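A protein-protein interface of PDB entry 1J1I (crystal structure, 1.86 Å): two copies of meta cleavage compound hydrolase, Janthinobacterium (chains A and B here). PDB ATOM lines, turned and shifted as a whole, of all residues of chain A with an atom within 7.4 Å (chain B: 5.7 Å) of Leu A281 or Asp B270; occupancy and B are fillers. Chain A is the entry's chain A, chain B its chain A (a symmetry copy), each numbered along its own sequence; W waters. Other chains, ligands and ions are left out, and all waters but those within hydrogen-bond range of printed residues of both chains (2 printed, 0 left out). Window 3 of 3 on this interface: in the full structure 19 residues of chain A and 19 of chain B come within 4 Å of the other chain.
NE1 of Trp A252 sits at hydrogen-bond distance from OD1 of Asp B270, 2.8 Å away.
The side-chain hydroxyl of Tyr B254 is in hydrogen-bond range of the side-chain carboxylate of Asp B270 (2.6 Å).
The backbone carbonyl oxygen of Ser A277 lies within hydrogen-bond range of the side-chain hydroxyl of Ser A280, 2.6 Å away.
O of Glu B269 lies close to OD1 of Asn B273 (3.3 Å).
Tyr B254 touches Trp A252.
Ile B256 touches Trp A252 (CG2 to NE1, 3.7 Å).
CB of Asn B273 touches OG of Ser A277 (3.7 Å).
Ser A280 touches Asn B273 (OG to ND2, 3.5 Å).
Leu A281 touches Asp B270 (CD1 to OD2, 3.2 Å).
Leu A281 touches just one residue of chain B: Asp B270 (3.2 Å).
Asp B270 touches just these residues of chain A: Trp A252 (2.8 Å) and Leu A281 (3.2 Å).
Of the printed residues of chain A, Ile B256 touches Trp A252 (3.7 Å).
Printed residues of chain B within 4 Å of Ser A280: Asn B273.
Printed residues of chain B within 4 Å of Trp A252: Tyr B254, Ile B256 and Asp B270.
Of the printed residues of chain B, Ser A277 touches Asn B273.
Printed residues of chain A within 4 Å of Tyr B254: Trp A252 (3.2 Å).
Ala B272 touches none of the printed residues of chain A.
Ala B274 touches none of the printed residues of chain A.
The nearest residue of chain B that does not touch Leu A281 is Glu B269 (4.2 Å).
Of the 10 printed residues of chain A, 4 touch a printed residue of chain B.
Hydrophobic or aromatic side chains of chain A within 4 Å of the printed part of chain B: Trp A252 and Leu A281.
Of the 11 printed residues of chain B, 4 touch a printed residue of chain A.
Hydrophobic or aromatic side chains of chain B within 4 Å of the printed part of chain A: Tyr B254 and Ile B256.
1 position is printed for both chains.
Water W2 lies within hydrogen-bond range of the side-chain hydroxyl (OH) of Tyr B254 and the backbone NH (N) of Phe A278.
Water W1 lies within hydrogen-bond range of the backbone carbonyl oxygen (O) of Asp B270 (2.8 Å), the side-chain hydroxyl (OG) of Ser A277 (3.0 Å) and the backbone NH (N) of Ala B274 (3.4 Å).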
ATOM      1  N   TYR A  66      14.504  10.414 -34.976  1.00  0.00           N
ATOM      2  CA  TYR A  66      14.779   8.981 -34.870  1.00  0.00           C
ATOM      3  C   TYR A  66      14.681   8.250 -36.200  1.00  0.00           C
ATOM      4  O   TYR A  66      14.193   8.793 -37.190  1.00  0.00           O
ATOM      5  CB  TYR A  66      13.782   8.307 -33.917  1.00  0.00           C
ATOM      6  CG  TYR A  66      13.783   8.842 -32.512  1.00  0.00           C
ATOM      7  CD1 TYR A  66      13.015   9.953 -32.164  1.00  0.00           C
ATOM      8  CD2 TYR A  66      14.594   8.267 -31.537  1.00  0.00           C
ATOM      9  CE1 TYR A  66      13.059  10.480 -30.874  1.00  0.00           C
ATOM     10  CE2 TYR A  66      14.647   8.784 -30.247  1.00  0.00           C
ATOM     11  CZ  TYR A  66      13.881   9.892 -29.923  1.00  0.00           C
ATOM     12  OH  TYR A  66      13.957  10.417 -28.657  1.00  0.00           O
ATOM     13  N   TRP A 252       3.731   5.926 -17.823  1.00  0.00           N
ATOM     14  CA  TRP A 252       3.318   7.325 -17.813  1.00  0.00           C
ATOM     15  C   TRP A 252       1.981   7.295 -18.535  1.00  0.00           C
ATOM     16  O   TRP A 252       1.711   6.367 -19.301  1.00  0.00           O
ATOM     17  CB  TRP A 252       4.290   8.176 -18.624  1.00  0.00           C
ATOM     18  CG  TRP A 252       5.507   8.652 -17.898  1.00  0.00           C
ATOM     19  CD1 TRP A 252       5.735   9.916 -17.426  1.00  0.00           C
ATOM     20  CD2 TRP A 252       6.691   7.896 -17.606  1.00  0.00           C
ATOM     21  NE1 TRP A 252       6.986   9.997 -16.867  1.00  0.00           N
ATOM     22  CE2 TRP A 252       7.599   8.773 -16.966  1.00  0.00           C
ATOM     23  CE3 TRP A 252       7.079   6.565 -17.832  1.00  0.00           C
ATOM     24  CZ2 TRP A 252       8.865   8.361 -16.537  1.00  0.00           C
ATOM     25  CZ3 TRP A 252       8.343   6.153 -17.406  1.00  0.00           C
ATOM     26  CH2 TRP A 252       9.222   7.052 -16.770  1.00  0.00           C
ATOM     27  N   THR A 275       4.941  11.655 -28.102  1.00  0.00           N
ATOM     28  CA  THR A 275       5.833  10.509 -28.247  1.00  0.00           C
ATOM     29  C   THR A 275       7.292  10.962 -28.235  1.00  0.00           C
ATOM     30  O   THR A 275       8.137  10.330 -27.602  1.00  0.00           O
ATOM     31  CB  THR A 275       5.553   9.746 -29.552  1.00  0.00           C
ATOM     32  OG1 THR A 275       4.209   9.246 -29.530  1.00  0.00           O
ATOM     33  CG2 THR A 275       6.525   8.578 -29.712  1.00  0.00           C
ATOM     34  N   LEU A 276       7.588  12.056 -28.934  1.00  0.00           N
ATOM     35  CA  LEU A 276       8.951  12.576 -28.969  1.00  0.00           C
ATOM     36  C   LEU A 276       9.397  12.934 -27.560  1.00  0.00           C
ATOM     37  O   LEU A 276      10.508  12.611 -27.149  1.00  0.00           O
ATOM     38  CB  LEU A 276       9.035  13.825 -29.854  1.00  0.00           C
ATOM     39  CG  LEU A 276       8.964  13.604 -31.365  1.00  0.00           C
ATOM     40  CD1 LEU A 276       8.942  14.946 -32.085  1.00  0.00           C
ATOM     41  CD2 LEU A 276      10.159  12.776 -31.812  1.00  0.00           C
ATOM     42  N   SER A 277       8.516  13.603 -26.827  1.00  0.00           N
ATOM     43  CA  SER A 277       8.800  14.019 -25.461  1.00  0.00           C
ATOM     44  C   SER A 277       9.089  12.799 -24.582  1.00  0.00           C
ATOM     45  O   SER A 277      10.064  12.779 -23.829  1.00  0.00           O
ATOM     46  CB  SER A 277       7.609  14.813 -24.910  1.00  0.00           C
ATOM     47  OG  SER A 277       7.868  15.326 -23.615  1.00  0.00           O
ATOM     48  N   PHE A 278       8.246  11.778 -24.688  1.00  0.00           N
ATOM     49  CA  PHE A 278       8.426  10.557 -23.907  1.00  0.00           C
ATOM     50  C   PHE A 278       9.767   9.891 -24.224  1.00  0.00           C
ATOM     51  O   PHE A 278      10.536   9.554 -23.322  1.00  0.00           O
ATOM     52  CB  PHE A 278       7.286   9.580 -24.197  1.00  0.00           C
ATOM     53  CG  PHE A 278       7.448   8.240 -23.529  1.00  0.00           C
ATOM     54  CD1 PHE A 278       7.461   8.132 -22.139  1.00  0.00           C
ATOM     55  CD2 PHE A 278       7.567   7.083 -24.291  1.00  0.00           C
ATOM     56  CE1 PHE A 278       7.589   6.886 -21.520  1.00  0.00           C
ATOM     57  CE2 PHE A 278       7.695   5.831 -23.681  1.00  0.00           C
ATOM     58  CZ  PHE A 278       7.706   5.733 -22.294  1.00  0.00           C
ATOM     59  N   LEU A 279      10.047   9.712 -25.510  1.00  0.00           N
ATOM     60  CA  LEU A 279      11.292   9.081 -25.932  1.00  0.00           C
ATOM     61  C   LEU A 279      12.548   9.879 -25.566  1.00  0.00           C
ATOM     62  O   LEU A 279      13.608   9.295 -25.345  1.00  0.00           O
ATOM     63  CB  LEU A 279      11.263   8.830 -27.443  1.00  0.00           C
ATOM     64  CG  LEU A 279      10.176   7.867 -27.923  1.00  0.00           C
ATOM     65  CD1 LEU A 279      10.194   7.792 -29.442  1.00  0.00           C
ATOM     66  CD2 LEU A 279      10.400   6.490 -27.306  1.00  0.00           C
ATOM     67  N   SER A 280      12.430  11.203 -25.488  1.00  0.00           N
ATOM     68  CA  SER A 280      13.580  12.042 -25.159  1.00  0.00           C
ATOM     69  C   SER A 280      14.074  11.800 -23.738  1.00  0.00           C
ATOM     70  O   SER A 280      15.261  11.943 -23.456  1.00  0.00           O
ATOM     71  CB  SER A 280      13.239  13.526 -25.332  1.00  0.00           C
ATOM     72  OG  SER A 280      12.310  13.950 -24.351  1.00  0.00           O
ATOM     73  N   LEU A 281      13.162  11.438 -22.843  1.00  0.00           N
ATOM     74  CA  LEU A 281      13.528  11.168 -21.459  1.00  0.00           C
ATOM     75  C   LEU A 281      14.163   9.790 -21.358  1.00  0.00           C
ATOM     76  O   LEU A 281      15.104   9.587 -20.596  1.00  0.00           O
ATOM     77  CB  LEU A 281      12.296  11.214 -20.554  1.00  0.00           C
ATOM     78  CG  LEU A 281      11.541  12.537 -20.416  1.00  0.00           C
ATOM     79  CD1 LEU A 281      10.327  12.320 -19.522  1.00  0.00           C
ATOM     80  CD2 LEU A 281      12.458  13.611 -19.837  1.00  0.00           C
ATOM     81  N   ARG A 282      13.634   8.847 -22.134  1.00  0.00           N
ATOM     82  CA  ARG A 282      14.128   7.473 -22.131  1.00  0.00           C
ATOM     83  C   ARG A 282      15.300   7.273 -23.086  1.00  0.00           C
ATOM     84  O   ARG A 282      15.673   8.242 -23.781  1.00  0.00           O
ATOM     85  CB  ARG A 282      12.993   6.513 -22.503  1.00  0.00           C
ATOM     86  CG  ARG A 282      11.708   6.731 -21.710  1.00  0.00           C
ATOM     87  CD  ARG A 282      11.978   6.777 -20.212  1.00  0.00           C
ATOM     88  NE  ARG A 282      11.589   8.058 -19.632  1.00  0.00           N
ATOM     89  CZ  ARG A 282      11.864   8.433 -18.387  1.00  0.00           C
ATOM     90  NH1 ARG A 282      12.536   7.622 -17.578  1.00  0.00           N
ATOM     91  NH2 ARG A 282      11.466   9.621 -17.947  1.00  0.00           N
ATOM     92  N   TYR B 254      -1.585  14.034 -17.965  1.00  0.00           N
ATOM     93  CA  TYR B 254      -0.208  13.533 -17.987  1.00  0.00           C
ATOM     94  C   TYR B 254       0.070  12.925 -16.619  1.00  0.00           C
ATOM     95  O   TYR B 254       0.245  13.638 -15.625  1.00  0.00           O
ATOM     96  CB  TYR B 254       0.800  14.650 -18.275  1.00  0.00           C
ATOM     97  CG  TYR B 254       2.211  14.138 -18.505  1.00  0.00           C
ATOM     98  CD1 TYR B 254       2.476  13.204 -19.506  1.00  0.00           C
ATOM     99  CD2 TYR B 254       3.276  14.569 -17.710  1.00  0.00           C
ATOM    100  CE1 TYR B 254       3.756  12.706 -19.713  1.00  0.00           C
ATOM    101  CE2 TYR B 254       4.568  14.078 -17.910  1.00  0.00           C
ATOM    102  CZ  TYR B 254       4.796  13.142 -18.914  1.00  0.00           C
ATOM    103  OH  TYR B 254       6.054  12.624 -19.111  1.00  0.00           O
ATOM    104  N   ILE B 256       2.434  10.674 -14.182  1.00  0.00           N
ATOM    105  CA  ILE B 256       3.838  10.331 -13.984  1.00  0.00           C
ATOM    106  C   ILE B 256       4.060   9.297 -12.879  1.00  0.00           C
ATOM    107  O   ILE B 256       3.575   9.454 -11.755  1.00  0.00           O
ATOM    108  CB  ILE B 256       4.644  11.604 -13.628  1.00  0.00           C
ATOM    109  CG1 ILE B 256       4.427  12.678 -14.698  1.00  0.00           C
ATOM    110  CG2 ILE B 256       6.121  11.280 -13.485  1.00  0.00           C
ATOM    111  CD1 ILE B 256       5.058  14.031 -14.338  1.00  0.00           C
ATOM    112  N   HIS B 267      10.992  15.701 -10.822  1.00  0.00           N
ATOM    113  CA  HIS B 267      11.388  15.363 -12.185  1.00  0.00           C
ATOM    114  C   HIS B 267      11.263  16.615 -13.041  1.00  0.00           C
ATOM    115  O   HIS B 267      10.388  16.698 -13.904  1.00  0.00           O
ATOM    116  CB  HIS B 267      10.471  14.267 -12.740  1.00  0.00           C
ATOM    117  CG  HIS B 267      10.361  13.063 -11.857  1.00  0.00           C
ATOM    118  ND1 HIS B 267      11.383  12.148 -11.715  1.00  0.00           N
ATOM    119  CD2 HIS B 267       9.355  12.629 -11.063  1.00  0.00           C
ATOM    120  CE1 HIS B 267      11.007  11.200 -10.874  1.00  0.00           C
ATOM    121  NE2 HIS B 267       9.781  11.470 -10.463  1.00  0.00           N
ATOM    122  N   PRO B 268      12.146  17.604 -12.820  1.00  0.00           N
ATOM    123  CA  PRO B 268      12.100  18.857 -13.583  1.00  0.00           C
ATOM    124  C   PRO B 268      12.133  18.741 -15.106  1.00  0.00           C
ATOM    125  O   PRO B 268      11.323  19.370 -15.790  1.00  0.00           O
ATOM    126  CB  PRO B 268      13.275  19.663 -13.007  1.00  0.00           C
ATOM    127  CG  PRO B 268      14.226  18.602 -12.521  1.00  0.00           C
ATOM    128  CD  PRO B 268      13.308  17.574 -11.910  1.00  0.00           C
ATOM    129  N   GLU B 269      13.053  17.938 -15.636  1.00  0.00           N
ATOM    130  CA  GLU B 269      13.159  17.765 -17.083  1.00  0.00           C
ATOM    131  C   GLU B 269      11.884  17.164 -17.665  1.00  0.00           C
ATOM    132  O   GLU B 269      11.384  17.608 -18.704  1.00  0.00           O
ATOM    133  CB  GLU B 269      14.347  16.866 -17.421  1.00  0.00           C
ATOM    134  CG  GLU B 269      15.698  17.508 -17.160  1.00  0.00           C
ATOM    135  CD  GLU B 269      16.462  17.786 -18.443  1.00  0.00           C
ATOM    136  OE1 GLU B 269      16.841  16.815 -19.137  1.00  0.00           O
ATOM    137  OE2 GLU B 269      16.681  18.976 -18.760  1.00  0.00           O
ATOM    138  N   ASP B 270      11.368  16.145 -16.989  1.00  0.00           N
ATOM    139  CA  ASP B 270      10.155  15.476 -17.429  1.00  0.00           C
ATOM    140  C   ASP B 270       9.000  16.478 -17.437  1.00  0.00           C
ATOM    141  O   ASP B 270       8.305  16.632 -18.437  1.00  0.00           O
ATOM    142  CB  ASP B 270       9.840  14.299 -16.495  1.00  0.00           C
ATOM    143  CG  ASP B 270       8.650  13.473 -16.970  1.00  0.00           C
ATOM    144  OD1 ASP B 270       8.365  12.424 -16.355  1.00  0.00           O
ATOM    145  OD2 ASP B 270       8.001  13.874 -17.953  1.00  0.00           O
ATOM    146  N   PHE B 271       8.808  17.171 -16.322  1.00  0.00           N
ATOM    147  CA  PHE B 271       7.730  18.145 -16.229  1.00  0.00           C
ATOM    148  C   PHE B 271       7.842  19.285 -17.239  1.00  0.00           C
ATOM    149  O   PHE B 271       6.852  19.653 -17.877  1.00  0.00           O
ATOM    150  CB  PHE B 271       7.664  18.755 -14.829  1.00  0.00           C
ATOM    151  CG  PHE B 271       6.641  19.842 -14.714  1.00  0.00           C
ATOM    152  CD1 PHE B 271       5.299  19.532 -14.493  1.00  0.00           C
ATOM    153  CD2 PHE B 271       7.000  21.171 -14.915  1.00  0.00           C
ATOM    154  CE1 PHE B 271       4.328  20.532 -14.488  1.00  0.00           C
ATOM    155  CE2 PHE B 271       6.036  22.175 -14.911  1.00  0.00           C
ATOM    156  CZ  PHE B 271       4.698  21.854 -14.696  1.00  0.00           C
ATOM    157  N   ALA B 272       9.037  19.856 -17.359  1.00  0.00           N
ATOM    158  CA  ALA B 272       9.274  20.968 -18.269  1.00  0.00           C
ATOM    159  C   ALA B 272       8.987  20.596 -19.715  1.00  0.00           C
ATOM    160  O   ALA B 272       8.390  21.376 -20.455  1.00  0.00           O
ATOM    161  CB  ALA B 272      10.717  21.462 -18.136  1.00  0.00           C
ATOM    162  N   ASN B 273       9.429  19.410 -20.114  1.00  0.00           N
ATOM    163  CA  ASN B 273       9.218  18.941 -21.475  1.00  0.00           C
ATOM    164  C   ASN B 273       7.749  18.676 -21.761  1.00  0.00           C
ATOM    165  O   ASN B 273       7.258  18.996 -22.839  1.00  0.00           O
ATOM    166  CB  ASN B 273      10.042  17.678 -21.730  1.00  0.00           C
ATOM    167  CG  ASN B 273      11.433  17.992 -22.245  1.00  0.00           C
ATOM    168  OD1 ASN B 273      12.123  18.865 -21.719  1.00  0.00           O
ATOM    169  ND2 ASN B 273      11.853  17.273 -23.277  1.00  0.00           N
ATOM    170  N   ALA B 274       7.049  18.095 -20.794  1.00  0.00           N
ATOM    171  CA  ALA B 274       5.631  17.809 -20.961  1.00  0.00           C
ATOM    172  C   ALA B 274       4.879  19.130 -21.117  1.00  0.00           C
ATOM    173  O   ALA B 274       3.915  19.229 -21.888  1.00  0.00           O
ATOM    174  CB  ALA B 274       5.105  17.044 -19.751  1.00  0.00           C
ATOM    175  N   THR B 275       5.326  20.144 -20.381  1.00  0.00           N
ATOM    176  CA  THR B 275       4.706  21.464 -20.441  1.00  0.00           C
ATOM    177  C   THR B 275       5.009  22.136 -21.779  1.00  0.00           C
ATOM    178  O   THR B 275       4.128  22.745 -22.384  1.00  0.00           O
ATOM    179  CB  THR B 275       5.204  22.364 -19.299  1.00  0.00           C
ATOM    180  OG1 THR B 275       4.847  21.778 -18.041  1.00  0.00           O
ATOM    181  CG2 THR B 275       4.582  23.757 -19.403  1.00  0.00           C
HETATM  182  O   HOH W   1       8.247  14.951 -20.684  1.00  0.00           O
HETATM  183  O   HOH W   2       6.890  12.271 -21.629  1.00  0.00           O
